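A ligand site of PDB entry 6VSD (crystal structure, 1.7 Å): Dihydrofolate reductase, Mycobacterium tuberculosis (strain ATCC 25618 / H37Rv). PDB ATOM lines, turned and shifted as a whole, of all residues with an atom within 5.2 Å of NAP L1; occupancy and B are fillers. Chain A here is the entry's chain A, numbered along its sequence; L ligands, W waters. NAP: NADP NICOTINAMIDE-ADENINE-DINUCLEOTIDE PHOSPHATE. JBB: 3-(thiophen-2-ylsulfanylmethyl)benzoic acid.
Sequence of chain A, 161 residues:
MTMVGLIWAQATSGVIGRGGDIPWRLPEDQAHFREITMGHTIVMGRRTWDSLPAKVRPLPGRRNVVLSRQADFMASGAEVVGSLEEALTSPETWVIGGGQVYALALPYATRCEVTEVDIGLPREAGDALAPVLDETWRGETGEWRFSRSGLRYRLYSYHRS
N of Arg 69 is in hydrogen-bond range of O3X of NAP L1, 2.6 Å away. The backbone NH of Thr 48 lies within hydrogen-bond range of an oxygen (O2A) of NAP L1 (3.1 Å). The side-chain hydroxyl (OG1) of Thr 48 is in hydrogen-bond range of an oxygen (O2A) of NAP L1. An oxygen (O5B) of NAP L1 sits at hydrogen-bond distance from the backbone NH of Arg 46. The guanidinium group of Arg 46 lies within salt-bridge range of an oxygen (O2X) of NAP L1 (2.8 Å). An oxygen (O2X) of NAP L1 lies within hydrogen-bond range of the side-chain hydroxyl (OG) of Ser 68. N of Gln 100 sits at hydrogen-bond distance from O2N of NAP L1, 2.9 Å away. The backbone NH of Gly 98 lies within hydrogen-bond range of an oxygen (O2A) of NAP L1 (2.9 Å). The backbone NH of Gly 99 lies within hydrogen-bond range of an oxygen (O2N) of NAP L1, 3.0 Å away. N of Asp 21 is in hydrogen-bond range of O3D of NAP L1, at 3.2 Å. O3D of NAP L1 sits at hydrogen-bond distance from O of Asp 21 (3.0 Å). The side-chain amide oxygen of Gln 70 lies close to an oxygen (O2X) of NAP L1, 3.1 Å away. The backbone carbonyl oxygen of Gly 20 is in hydrogen-bond range of an oxygen (O2D) of NAP L1, 3.4 Å away. O5B of NAP L1 sits at hydrogen-bond distance from N of Arg 47, at 3.4 Å. The guanidinium group of Arg 47 lies within salt-bridge range of an oxygen (O1N) of NAP L1. The backbone NH of Val 101 is in hydrogen-bond range of an oxygen (O1A) of NAP L1 (3.4 Å).
N of Gly 98 lies within hydrogen-bond range of OG1 of Thr 48, at 3.0 Å. The backbone carbonyl oxygen (O) of Leu 67 sits at hydrogen-bond distance from the backbone NH (N) of Arg 46 (3.1 Å). The side-chain hydroxyl (OG) of Ser 68 is in hydrogen-bond range of the backbone NH (N) of Gln 70, at 2.9 Å. O of Ile 96 lies close to OH of Tyr 102, at 3.3 Å. N of Gly 45 lies within hydrogen-bond range of O of Gly 97, 2.9 Å away. NE1 of Trp 8 sits at hydrogen-bond distance from OE1 of Gln 10, at 3.0 Å. N of Gly 97 lies close to OH of Tyr 102. The backbone carbonyl oxygen (O) of Gly 17 is in hydrogen-bond range of the backbone NH (N) of Ala 128.
The backbone carbonyl oxygen of Ala 9 sits close to an oxygen (O7N) of NAP L1 (2.9 Å). An oxygen (O7N) of NAP L1 sits close to the backbone carbonyl oxygen of Ile 16, 2.9 Å away. O4B of NAP L1 lies close to O of Leu 67 (3.4 Å). Trp 8 touches NAP L1 (CA to N7N, 3.4 Å). Gly 17 touches NAP L1. Arg 18 touches NAP L1 (N to O3D, 3.8 Å). Ile 22 touches NAP L1. CA of Gly 45 touches O5B of NAP L1, 3.2 Å away. O of Gly 82 touches C2A of NAP L1, at 3.4 Å. Ile 96 touches NAP L1. Gly 97 touches NAP L1. Tyr 102 touches NAP L1 (OH to C4N, 3.6 Å). CD2 of Leu 104 touches N6A of NAP L1, 3.6 Å away. Ala 128 touches NAP L1. Hydrophobic or aromatic side chains within 4 Å of NAP L1: Trp 8, Ile 16, Ile 22, Leu 67, Val 101, Leu 104 and Ala 128. 26 residues have an atom within 4 Å of NAP L1: Trp 8, Ala 9, Ile 16, Gly 17, Arg 18, Gly 20, Asp 21, Ile 22, Gly 45, Arg 46, Arg 47, Thr 48, Leu 67, Ser 68, Arg 69, Gln 70, Gly 82, Ile 96, Gly 97, Gly 98, Gly 99, Gln 100, Val 101, Tyr 102, Leu 104 and Ala 128. Along chain A the residues within 4 Å of NAP L1 span positions 8 to 128. The nearest printed residue that does not touch NAP L1 is Trp 24 (4.1 Å).
Water W5 bridges the guanidinium group of Arg 69 (2.9 Å) and an oxygen (O3X) of NAP L1 (3.0 Å).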
ATOM      1  N   ILE A   7     -25.628  24.121  -9.869  1.00  0.00           N
ATOM      2  CA  ILE A   7     -25.017  25.334 -10.398  1.00  0.00           C
ATOM      3  C   ILE A   7     -23.806  24.955 -11.240  1.00  0.00           C
ATOM      4  O   ILE A   7     -22.961  24.160 -10.798  1.00  0.00           O
ATOM      5  CB  ILE A   7     -24.653  26.316  -9.265  1.00  0.00           C
ATOM      6  CG1 ILE A   7     -24.082  27.628  -9.826  1.00  0.00           C
ATOM      7  CG2 ILE A   7     -23.729  25.649  -8.237  1.00  0.00           C
ATOM      8  CD1 ILE A   7     -24.071  28.762  -8.811  1.00  0.00           C
ATOM      9  N   TRP A   8     -23.728  25.491 -12.453  1.00  0.00           N
ATOM     10  CA  TRP A   8     -22.639  25.178 -13.358  1.00  0.00           C
ATOM     11  C   TRP A   8     -22.517  26.270 -14.397  1.00  0.00           C
ATOM     12  O   TRP A   8     -23.414  27.108 -14.552  1.00  0.00           O
ATOM     13  CB  TRP A   8     -22.839  23.797 -14.020  1.00  0.00           C
ATOM     14  CG  TRP A   8     -23.821  23.702 -15.153  1.00  0.00           C
ATOM     15  CD1 TRP A   8     -23.620  24.088 -16.445  1.00  0.00           C
ATOM     16  CD2 TRP A   8     -25.145  23.143 -15.103  1.00  0.00           C
ATOM     17  NE1 TRP A   8     -24.734  23.812 -17.212  1.00  0.00           N
ATOM     18  CE2 TRP A   8     -25.685  23.234 -16.403  1.00  0.00           C
ATOM     19  CE3 TRP A   8     -25.913  22.579 -14.092  1.00  0.00           C
ATOM     20  CZ2 TRP A   8     -26.976  22.797 -16.708  1.00  0.00           C
ATOM     21  CZ3 TRP A   8     -27.205  22.129 -14.398  1.00  0.00           C
ATOM     22  CH2 TRP A   8     -27.713  22.246 -15.700  1.00  0.00           C
ATOM     23  N   ALA A   9     -21.388  26.267 -15.103  1.00  0.00           N
ATOM     24  CA  ALA A   9     -21.162  27.088 -16.285  1.00  0.00           C
ATOM     25  C   ALA A   9     -20.834  26.175 -17.452  1.00  0.00           C
ATOM     26  O   ALA A   9     -20.146  25.171 -17.277  1.00  0.00           O
ATOM     27  CB  ALA A   9     -20.028  28.089 -16.074  1.00  0.00           C
ATOM     28  N   GLN A  10     -21.332  26.499 -18.636  1.00  0.00           N
ATOM     29  CA  GLN A  10     -21.135  25.644 -19.791  1.00  0.00           C
ATOM     30  C   GLN A  10     -20.810  26.470 -21.015  1.00  0.00           C
ATOM     31  O   GLN A  10     -21.224  27.619 -21.133  1.00  0.00           O
ATOM     32  CB  GLN A  10     -22.371  24.793 -20.062  1.00  0.00           C
ATOM     33  CG  GLN A  10     -23.590  25.553 -20.524  1.00  0.00           C
ATOM     34  CD  GLN A  10     -24.690  24.616 -20.940  1.00  0.00           C
ATOM     35  OE1 GLN A  10     -25.312  23.961 -20.103  1.00  0.00           O
ATOM     36  NE2 GLN A  10     -24.931  24.521 -22.235  1.00  0.00           N
ATOM     37  N   ILE A  16     -18.646  21.347 -19.910  1.00  0.00           N
ATOM     38  CA  ILE A  16     -18.391  21.999 -18.630  1.00  0.00           C
ATOM     39  C   ILE A  16     -16.985  21.746 -18.101  1.00  0.00           C
ATOM     40  O   ILE A  16     -16.537  22.461 -17.192  1.00  0.00           O
ATOM     41  CB  ILE A  16     -19.427  21.571 -17.568  1.00  0.00           C
ATOM     42  CG1 ILE A  16     -19.214  20.116 -17.133  1.00  0.00           C
ATOM     43  CG2 ILE A  16     -20.859  21.790 -18.099  1.00  0.00           C
ATOM     44  CD1 ILE A  16     -19.962  19.735 -15.853  1.00  0.00           C
ATOM     45  N   GLY A  17     -16.258  20.760 -18.622  1.00  0.00           N
ATOM     46  CA  GLY A  17     -14.952  20.467 -18.114  1.00  0.00           C
ATOM     47  C   GLY A  17     -14.162  19.587 -19.113  1.00  0.00           C
ATOM     48  O   GLY A  17     -14.772  18.861 -19.890  1.00  0.00           O
ATOM     49  N   ARG A  18     -12.854  19.687 -19.006  1.00  0.00           N
ATOM     50  CA  ARG A  18     -11.961  19.006 -19.939  1.00  0.00           C
ATOM     51  C   ARG A  18     -10.584  18.856 -19.287  1.00  0.00           C
ATOM     52  O   ARG A  18     -10.004  19.839 -18.823  1.00  0.00           O
ATOM     53  CB  ARG A  18     -11.863  19.807 -21.238  1.00  0.00           C
ATOM     54  CG  ARG A  18     -10.803  19.339 -22.207  1.00  0.00           C
ATOM     55  CD  ARG A  18     -10.882  20.125 -23.505  1.00  0.00           C
ATOM     56  NE  ARG A  18     -12.143  19.878 -24.187  1.00  0.00           N
ATOM     57  CZ  ARG A  18     -12.580  20.554 -25.237  1.00  0.00           C
ATOM     58  NH1 ARG A  18     -11.846  21.528 -25.743  1.00  0.00           N
ATOM     59  NH2 ARG A  18     -13.740  20.243 -25.790  1.00  0.00           N
ATOM     60  N   GLY A  19     -10.087  17.630 -19.237  1.00  0.00           N
ATOM     61  CA  GLY A  19      -8.793  17.398 -18.633  1.00  0.00           C
ATOM     62  C   GLY A  19      -8.777  17.572 -17.133  1.00  0.00           C
ATOM     63  O   GLY A  19      -7.725  17.824 -16.554  1.00  0.00           O
ATOM     64  N   GLY A  20      -9.940  17.441 -16.486  1.00  0.00           N
ATOM     65  CA  GLY A  20     -10.037  17.639 -15.059  1.00  0.00           C
ATOM     66  C   GLY A  20     -10.192  19.078 -14.620  1.00  0.00           C
ATOM     67  O   GLY A  20     -10.296  19.315 -13.414  1.00  0.00           O
ATOM     68  N   ASP A  21     -10.207  20.030 -15.537  1.00  0.00           N
ATOM     69  CA  ASP A  21     -10.357  21.420 -15.177  1.00  0.00           C
ATOM     70  C   ASP A  21     -11.406  22.061 -16.094  1.00  0.00           C
ATOM     71  O   ASP A  21     -12.261  21.389 -16.672  1.00  0.00           O
ATOM     72  CB  ASP A  21      -9.007  22.141 -15.228  1.00  0.00           C
ATOM     73  CG  ASP A  21      -8.944  23.283 -14.252  1.00  0.00           C
ATOM     74  OD1 ASP A  21      -9.292  24.417 -14.661  1.00  0.00           O
ATOM     75  OD2 ASP A  21      -8.576  23.063 -13.085  1.00  0.00           O
ATOM     76  N   ILE A  22     -11.358  23.389 -16.196  1.00  0.00           N
ATOM     77  CA  ILE A  22     -12.337  24.185 -16.944  1.00  0.00           C
ATOM     78  C   ILE A  22     -11.597  25.070 -17.937  1.00  0.00           C
ATOM     79  O   ILE A  22     -10.658  25.793 -17.546  1.00  0.00           O
ATOM     80  CB  ILE A  22     -13.190  25.056 -16.015  1.00  0.00           C
ATOM     81  CG1 ILE A  22     -13.811  24.228 -14.906  1.00  0.00           C
ATOM     82  CG2 ILE A  22     -14.287  25.742 -16.785  1.00  0.00           C
ATOM     83  CD1 ILE A  22     -14.530  25.091 -13.925  1.00  0.00           C
ATOM     84  N   TRP A  24     -11.939  27.929 -19.111  1.00  0.00           N
ATOM     85  CA  TRP A  24     -12.162  29.366 -19.003  1.00  0.00           C
ATOM     86  C   TRP A  24     -12.109  29.735 -17.541  1.00  0.00           C
ATOM     87  O   TRP A  24     -12.065  28.870 -16.661  1.00  0.00           O
ATOM     88  CB  TRP A  24     -13.492  29.788 -19.617  1.00  0.00           C
ATOM     89  CG  TRP A  24     -14.674  29.178 -18.951  1.00  0.00           C
ATOM     90  CD1 TRP A  24     -15.270  29.567 -17.764  1.00  0.00           C
ATOM     91  CD2 TRP A  24     -15.416  28.050 -19.417  1.00  0.00           C
ATOM     92  NE1 TRP A  24     -16.337  28.757 -17.488  1.00  0.00           N
ATOM     93  CE2 TRP A  24     -16.440  27.806 -18.483  1.00  0.00           C
ATOM     94  CE3 TRP A  24     -15.308  27.219 -20.543  1.00  0.00           C
ATOM     95  CZ2 TRP A  24     -17.362  26.763 -18.644  1.00  0.00           C
ATOM     96  CZ3 TRP A  24     -16.218  26.187 -20.685  1.00  0.00           C
ATOM     97  CH2 TRP A  24     -17.223  25.970 -19.746  1.00  0.00           C
ATOM     98  N   GLY A  45     -18.403  15.974  -6.737  1.00  0.00           N
ATOM     99  CA  GLY A  45     -17.781  14.699  -6.958  1.00  0.00           C
ATOM    100  C   GLY A  45     -16.317  14.722  -6.580  1.00  0.00           C
ATOM    101  O   GLY A  45     -15.701  15.775  -6.446  1.00  0.00           O
ATOM    102  N   ARG A  46     -15.741  13.532  -6.384  1.00  0.00           N
ATOM    103  CA  ARG A  46     -14.347  13.463  -5.970  1.00  0.00           C
ATOM    104  C   ARG A  46     -13.436  14.131  -6.985  1.00  0.00           C
ATOM    105  O   ARG A  46     -12.460  14.802  -6.600  1.00  0.00           O
ATOM    106  CB  ARG A  46     -13.942  12.004  -5.744  1.00  0.00           C
ATOM    107  CG  ARG A  46     -12.618  11.839  -4.997  1.00  0.00           C
ATOM    108  CD  ARG A  46     -11.469  11.664  -5.959  1.00  0.00           C
ATOM    109  NE  ARG A  46     -11.734  10.539  -6.834  1.00  0.00           N
ATOM    110  CZ  ARG A  46     -11.141  10.348  -8.001  1.00  0.00           C
ATOM    111  NH1 ARG A  46     -10.242  11.217  -8.439  1.00  0.00           N
ATOM    112  NH2 ARG A  46     -11.444   9.297  -8.741  1.00  0.00           N
ATOM    113  N   ARG A  47     -13.712  13.973  -8.271  1.00  0.00           N
ATOM    114  CA  ARG A  47     -12.862  14.597  -9.295  1.00  0.00           C
ATOM    115  C   ARG A  47     -12.901  16.109  -9.206  1.00  0.00           C
ATOM    116  O   ARG A  47     -11.879  16.777  -9.398  1.00  0.00           O
ATOM    117  CB  ARG A  47     -13.282  14.119 -10.688  1.00  0.00           C
ATOM    118  CG  ARG A  47     -12.909  12.698 -10.979  1.00  0.00           C
ATOM    119  CD  ARG A  47     -13.393  12.316 -12.359  1.00  0.00           C
ATOM    120  NE  ARG A  47     -12.862  11.029 -12.807  1.00  0.00           N
ATOM    121  CZ  ARG A  47     -13.188  10.462 -13.967  1.00  0.00           C
ATOM    122  NH1 ARG A  47     -14.035  11.071 -14.792  1.00  0.00           N
ATOM    123  NH2 ARG A  47     -12.666   9.298 -14.300  1.00  0.00           N
ATOM    124  N   THR A  48     -14.066  16.673  -8.901  1.00  0.00           N
ATOM    125  CA  THR A  48     -14.176  18.119  -8.749  1.00  0.00           C
ATOM    126  C   THR A  48     -13.449  18.610  -7.486  1.00  0.00           C
ATOM    127  O   THR A  48     -12.786  19.643  -7.519  1.00  0.00           O
ATOM    128  CB  THR A  48     -15.645  18.532  -8.749  1.00  0.00           C
ATOM    129  OG1 THR A  48     -16.194  18.296 -10.059  1.00  0.00           O
ATOM    130  CG2 THR A  48     -15.799  20.009  -8.396  1.00  0.00           C
ATOM    131  N   SER A  51      -9.999  18.964  -8.288  1.00  0.00           N
ATOM    132  CA  SER A  51      -9.707  20.122  -9.134  1.00  0.00           C
ATOM    133  C   SER A  51      -9.534  21.419  -8.343  1.00  0.00           C
ATOM    134  O   SER A  51      -9.000  22.383  -8.891  1.00  0.00           O
ATOM    135  CB  SER A  51     -10.805  20.283 -10.189  1.00  0.00           C
ATOM    136  OG  SER A  51     -11.908  21.006  -9.686  1.00  0.00           O
ATOM    137  N   LEU A  67     -18.533  13.393  -2.818  1.00  0.00           N
ATOM    138  CA  LEU A  67     -19.125  12.102  -3.138  1.00  0.00           C
ATOM    139  C   LEU A  67     -18.067  11.200  -3.735  1.00  0.00           C
ATOM    140  O   LEU A  67     -17.491  11.518  -4.782  1.00  0.00           O
ATOM    141  CB  LEU A  67     -20.283  12.299  -4.098  1.00  0.00           C
ATOM    142  CG  LEU A  67     -21.126  11.106  -4.496  1.00  0.00           C
ATOM    143  CD1 LEU A  67     -21.809  10.507  -3.284  1.00  0.00           C
ATOM    144  CD2 LEU A  67     -22.134  11.615  -5.467  1.00  0.00           C
ATOM    145  N   SER A  68     -17.817  10.067  -3.077  1.00  0.00           N
ATOM    146  CA  SER A  68     -16.789   9.133  -3.490  1.00  0.00           C
ATOM    147  C   SER A  68     -17.250   7.709  -3.213  1.00  0.00           C
ATOM    148  O   SER A  68     -17.942   7.450  -2.232  1.00  0.00           O
ATOM    149  CB  SER A  68     -15.468   9.384  -2.759  1.00  0.00           C
ATOM    150  OG  SER A  68     -14.513   8.414  -3.115  1.00  0.00           O
ATOM    151  N   ARG A  69     -16.866   6.789  -4.100  1.00  0.00           N
ATOM    152  CA  ARG A  69     -17.050   5.383  -3.787  1.00  0.00           C
ATOM    153  C   ARG A  69     -15.896   4.803  -2.975  1.00  0.00           C
ATOM    154  O   ARG A  69     -16.009   3.675  -2.510  1.00  0.00           O
ATOM    155  CB  ARG A  69     -17.230   4.570  -5.075  1.00  0.00           C
ATOM    156  CG  ARG A  69     -18.501   4.901  -5.815  1.00  0.00           C
ATOM    157  CD  ARG A  69     -18.799   3.847  -6.856  1.00  0.00           C
ATOM    158  NE  ARG A  69     -20.006   4.154  -7.612  1.00  0.00           N
ATOM    159  CZ  ARG A  69     -20.023   4.952  -8.677  1.00  0.00           C
ATOM    160  NH1 ARG A  69     -18.898   5.514  -9.078  1.00  0.00           N
ATOM    161  NH2 ARG A  69     -21.148   5.191  -9.326  1.00  0.00           N
ATOM    162  N   GLN A  70     -14.809   5.566  -2.786  1.00  0.00           N
ATOM    163  CA  GLN A  70     -13.672   5.111  -1.992  1.00  0.00           C
ATOM    164  C   GLN A  70     -13.956   5.308  -0.510  1.00  0.00           C
ATOM    165  O   GLN A  70     -13.917   6.440  -0.004  1.00  0.00           O
ATOM    166  CB  GLN A  70     -12.399   5.873  -2.363  1.00  0.00           C
ATOM    167  CG  GLN A  70     -11.979   5.818  -3.806  1.00  0.00           C
ATOM    168  CD  GLN A  70     -10.751   6.699  -4.054  1.00  0.00           C
ATOM    169  OE1 GLN A  70     -10.735   7.495  -5.000  1.00  0.00           O
ATOM    170  NE2 GLN A  70      -9.746   6.572  -3.185  1.00  0.00           N
ATOM    171  N   GLY A  82     -20.629   8.267   0.502  1.00  0.00           N
ATOM    172  CA  GLY A  82     -20.687   7.308  -0.587  1.00  0.00           C
ATOM    173  C   GLY A  82     -22.004   7.274  -1.346  1.00  0.00           C
ATOM    174  O   GLY A  82     -22.154   6.513  -2.298  1.00  0.00           O
ATOM    175  N   SER A  83     -22.961   8.101  -0.918  1.00  0.00           N
ATOM    176  CA  SER A  83     -24.237   8.241  -1.604  1.00  0.00           C
ATOM    177  C   SER A  83     -24.694   9.692  -1.527  1.00  0.00           C
ATOM    178  O   SER A  83     -24.364  10.414  -0.599  1.00  0.00           O
ATOM    179  CB  SER A  83     -25.305   7.309  -1.002  1.00  0.00           C
ATOM    180  OG  SER A  83     -25.925   7.853   0.152  1.00  0.00           O
ATOM    181  N   ILE A  96     -22.294  21.248  -7.052  1.00  0.00           N
ATOM    182  CA  ILE A  96     -21.382  22.157  -7.733  1.00  0.00           C
ATOM    183  C   ILE A  96     -20.469  21.431  -8.730  1.00  0.00           C
ATOM    184  O   ILE A  96     -19.449  21.995  -9.131  1.00  0.00           O
ATOM    185  CB  ILE A  96     -20.557  22.976  -6.726  1.00  0.00           C
ATOM    186  CG1 ILE A  96     -19.577  22.066  -5.973  1.00  0.00           C
ATOM    187  CG2 ILE A  96     -21.480  23.667  -5.729  1.00  0.00           C
ATOM    188  CD1 ILE A  96     -18.435  22.814  -5.299  1.00  0.00           C
ATOM    189  N   GLY A  97     -20.811  20.211  -9.141  1.00  0.00           N
ATOM    190  CA  GLY A  97     -20.014  19.500 -10.130  1.00  0.00           C
ATOM    191  C   GLY A  97     -19.545  18.133  -9.684  1.00  0.00           C
ATOM    192  O   GLY A  97     -19.662  17.825  -8.506  1.00  0.00           O
ATOM    193  N   GLY A  98     -19.017  17.311 -10.589  1.00  0.00           N
ATOM    194  CA  GLY A  98     -18.849  17.647 -11.985  1.00  0.00           C
ATOM    195  C   GLY A  98     -19.943  17.003 -12.796  1.00  0.00           C
ATOM    196  O   GLY A  98     -21.067  16.902 -12.314  1.00  0.00           O
ATOM    197  N   GLY A  99     -19.643  16.531 -14.006  1.00  0.00           N
ATOM    198  CA  GLY A  99     -20.690  16.020 -14.880  1.00  0.00           C
ATOM    199  C   GLY A  99     -21.432  14.813 -14.325  1.00  0.00           C
ATOM    200  O   GLY A  99     -22.649  14.676 -14.487  1.00  0.00           O
ATOM    201  N   GLN A 100     -20.713  13.898 -13.683  1.00  0.00           N
ATOM    202  CA  GLN A 100     -21.335  12.699 -13.146  1.00  0.00           C
ATOM    203  C   GLN A 100     -22.327  13.048 -12.048  1.00  0.00           C
ATOM    204  O   GLN A 100     -23.452  12.547 -12.017  1.00  0.00           O
ATOM    205  CB  GLN A 100     -20.283  11.722 -12.614  1.00  0.00           C
ATOM    206  CG  GLN A 100     -19.349  11.230 -13.668  1.00  0.00           C
ATOM    207  CD  GLN A 100     -18.517  10.060 -13.183  1.00  0.00           C
ATOM    208  OE1 GLN A 100     -18.719   9.559 -12.080  1.00  0.00           O
ATOM    209  NE2 GLN A 100     -17.598   9.622 -14.013  1.00  0.00           N
ATOM    210  N   VAL A 101     -21.918  13.930 -11.139  1.00  0.00           N
ATOM    211  CA  VAL A 101     -22.740  14.224  -9.981  1.00  0.00           C
ATOM    212  C   VAL A 101     -23.923  15.094 -10.366  1.00  0.00           C
ATOM    213  O   VAL A 101     -24.997  14.990  -9.763  1.00  0.00           O
ATOM    214  CB  VAL A 101     -21.858  14.859  -8.895  1.00  0.00           C
ATOM    215  CG1 VAL A 101     -22.691  15.241  -7.684  1.00  0.00           C
ATOM    216  CG2 VAL A 101     -20.762  13.879  -8.491  1.00  0.00           C
ATOM    217  N   TYR A 102     -23.760  15.957 -11.369  1.00  0.00           N
ATOM    218  CA  TYR A 102     -24.915  16.665 -11.920  1.00  0.00           C
ATOM    219  C   TYR A 102     -25.977  15.683 -12.398  1.00  0.00           C
ATOM    220  O   TYR A 102     -27.144  15.774 -12.013  1.00  0.00           O
ATOM    221  CB  TYR A 102     -24.481  17.589 -13.063  1.00  0.00           C
ATOM    222  CG  TYR A 102     -23.721  18.837 -12.656  1.00  0.00           C
ATOM    223  CD1 TYR A 102     -24.074  19.563 -11.517  1.00  0.00           C
ATOM    224  CD2 TYR A 102     -22.668  19.317 -13.422  1.00  0.00           C
ATOM    225  CE1 TYR A 102     -23.392  20.722 -11.162  1.00  0.00           C
ATOM    226  CE2 TYR A 102     -21.972  20.470 -13.087  1.00  0.00           C
ATOM    227  CZ  TYR A 102     -22.338  21.163 -11.956  1.00  0.00           C
ATOM    228  OH  TYR A 102     -21.650  22.295 -11.620  1.00  0.00           O
ATOM    229  N   LEU A 104     -26.336  12.626 -11.561  1.00  0.00           N
ATOM    230  CA  LEU A 104     -26.815  11.843 -10.430  1.00  0.00           C
ATOM    231  C   LEU A 104     -27.826  12.644  -9.598  1.00  0.00           C
ATOM    232  O   LEU A 104     -28.765  12.072  -9.048  1.00  0.00           O
ATOM    233  CB  LEU A 104     -25.625  11.399  -9.583  1.00  0.00           C
ATOM    234  CG  LEU A 104     -25.855  10.568  -8.320  1.00  0.00           C
ATOM    235  CD1 LEU A 104     -26.368   9.172  -8.641  1.00  0.00           C
ATOM    236  CD2 LEU A 104     -24.592  10.516  -7.511  1.00  0.00           C
ATOM    237  N   ALA A 128     -16.412  16.521 -19.717  1.00  0.00           N
ATOM    238  CA  ALA A 128     -17.587  16.524 -18.859  1.00  0.00           C
ATOM    239  C   ALA A 128     -18.628  17.440 -19.486  1.00  0.00           C
ATOM    240  O   ALA A 128     -18.295  18.472 -20.063  1.00  0.00           O
ATOM    241  CB  ALA A 128     -17.239  16.991 -17.450  1.00  0.00           C
HETATM  242  PA  NAP L   1     -17.095  14.371 -10.860  1.00  0.00           P
HETATM  243  O1A NAP L   1     -18.523  14.224 -11.243  1.00  0.00           O
HETATM  244  O2A NAP L   1     -16.567  15.690 -10.363  1.00  0.00           O
HETATM  245  O5B NAP L   1     -16.737  13.286  -9.680  1.00  0.00           O
HETATM  246  C5B NAP L   1     -16.879  11.994 -10.223  1.00  0.00           C
HETATM  247  C4B NAP L   1     -16.594  11.085  -9.033  1.00  0.00           C
HETATM  248  O4B NAP L   1     -17.663  11.181  -8.115  1.00  0.00           O
HETATM  249  C3B NAP L   1     -16.441   9.628  -9.371  1.00  0.00           C
HETATM  250  O3B NAP L   1     -15.149   9.381  -9.847  1.00  0.00           O
HETATM  251  C2B NAP L   1     -16.594   9.050  -7.927  1.00  0.00           C
HETATM  252  O2B NAP L   1     -15.591   9.385  -7.102  1.00  0.00           O
HETATM  253  C1B NAP L   1     -17.786   9.918  -7.458  1.00  0.00           C
HETATM  254  N9A NAP L   1     -19.068   9.361  -7.832  1.00  0.00           N
HETATM  255  C8A NAP L   1     -19.732   9.473  -9.050  1.00  0.00           C
HETATM  256  N7A NAP L   1     -20.914   8.854  -9.063  1.00  0.00           N
HETATM  257  C5A NAP L   1     -21.035   8.299  -7.782  1.00  0.00           C
HETATM  258  C6A NAP L   1     -22.045   7.538  -7.152  1.00  0.00           C
HETATM  259  N6A NAP L   1     -23.196   7.175  -7.821  1.00  0.00           N
HETATM  260  N1A NAP L   1     -21.921   7.123  -5.869  1.00  0.00           N
HETATM  261  C2A NAP L   1     -20.757   7.512  -5.250  1.00  0.00           C
HETATM  262  N3A NAP L   1     -19.712   8.235  -5.698  1.00  0.00           N
HETATM  263  C4A NAP L   1     -19.877   8.627  -6.997  1.00  0.00           C
HETATM  264  O3  NAP L   1     -16.190  13.824 -12.171  1.00  0.00           O
HETATM  265  PN  NAP L   1     -16.512  14.449 -13.601  1.00  0.00           P
HETATM  266  O1N NAP L   1     -15.299  14.195 -14.414  1.00  0.00           O
HETATM  267  O2N NAP L   1     -17.887  14.145 -14.150  1.00  0.00           O
HETATM  268  O5D NAP L   1     -16.532  16.168 -13.526  1.00  0.00           O
HETATM  269  C5D NAP L   1     -15.233  16.634 -13.428  1.00  0.00           C
HETATM  270  C4D NAP L   1     -15.081  17.803 -14.414  1.00  0.00           C
HETATM  271  O4D NAP L   1     -16.147  18.795 -14.247  1.00  0.00           O
HETATM  272  C3D NAP L   1     -13.733  18.537 -14.130  1.00  0.00           C
HETATM  273  O3D NAP L   1     -13.188  18.896 -15.337  1.00  0.00           O
HETATM  274  C2D NAP L   1     -14.212  19.781 -13.395  1.00  0.00           C
HETATM  275  O2D NAP L   1     -13.364  20.841 -13.604  1.00  0.00           O
HETATM  276  C1D NAP L   1     -15.534  20.057 -14.184  1.00  0.00           C
HETATM  277  N1N NAP L   1     -16.395  20.993 -13.448  1.00  0.00           N
HETATM  278  C2N NAP L   1     -16.959  22.030 -14.133  1.00  0.00           C
HETATM  279  C3N NAP L   1     -17.793  22.912 -13.511  1.00  0.00           C
HETATM  280  C7N NAP L   1     -18.352  24.004 -14.306  1.00  0.00           C
HETATM  281  O7N NAP L   1     -18.092  24.260 -15.488  1.00  0.00           O
HETATM  282  N7N NAP L   1     -19.230  24.803 -13.673  1.00  0.00           N
HETATM  283  C4N NAP L   1     -18.136  22.777 -12.070  1.00  0.00           C
HETATM  284  C5N NAP L   1     -17.468  21.628 -11.413  1.00  0.00           C
HETATM  285  C6N NAP L   1     -16.664  20.802 -12.078  1.00  0.00           C
HETATM  286  P2B NAP L   1     -14.421   8.055  -6.745  1.00  0.00           P
HETATM  287  O1X NAP L   1     -13.932   7.891  -8.149  1.00  0.00           O
HETATM  288  O2X NAP L   1     -13.450   8.678  -5.732  1.00  0.00           O
HETATM  289  O3X NAP L   1     -15.404   7.055  -6.223  1.00  0.00           O
HETATM  290  C10 JBB L   2     -14.996  25.523  -8.221  1.00  0.00           C
HETATM  291  C13 JBB L   2     -15.324  23.692  -9.684  1.00  0.00           C
HETATM  292  C15 JBB L   2     -11.239  28.421  -6.831  1.00  0.00           C
HETATM  293  O01 JBB L   2     -10.993  30.368  -4.811  1.00  0.00           O
HETATM  294  C02 JBB L   2     -10.154  30.413  -5.755  1.00  0.00           C
HETATM  295  C03 JBB L   2     -10.346  29.461  -6.942  1.00  0.00           C
HETATM  296  C04 JBB L   2      -9.638  29.647  -8.115  1.00  0.00           C
HETATM  297  C05 JBB L   2      -9.842  28.782  -9.179  1.00  0.00           C
HETATM  298  C06 JBB L   2     -10.743  27.736  -9.065  1.00  0.00           C
HETATM  299  C07 JBB L   2     -11.442  27.584  -7.892  1.00  0.00           C
HETATM  300  C08 JBB L   2     -12.422  26.435  -7.761  1.00  0.00           C
HETATM  301  S09 JBB L   2     -14.136  26.912  -7.411  1.00  0.00           S
HETATM  302  S11 JBB L   2     -16.547  24.940  -7.935  1.00  0.00           S
HETATM  303  C12 JBB L   2     -16.570  23.667  -9.044  1.00  0.00           C
HETATM  304  C14 JBB L   2     -14.450  24.719  -9.225  1.00  0.00           C
HETATM  305  O16 JBB L   2      -9.194  31.222  -5.696  1.00  0.00           O
HETATM  306  O   HOH W   1     -11.562   5.636  -8.585  1.00  0.00           O
HETATM  307  O   HOH W   2     -22.715   8.117 -11.018  1.00  0.00           O
HETATM  308  O   HOH W   3     -25.660   4.888  -7.019  1.00  0.00           O
HETATM  309  O   HOH W   4     -18.020  13.249 -16.648  1.00  0.00           O
HETATM  310  O   HOH W   5     -16.086   5.255  -8.512  1.00  0.00           O
HETATM  311  O   HOH W   6     -19.240  26.460 -11.512  1.00  0.00           O
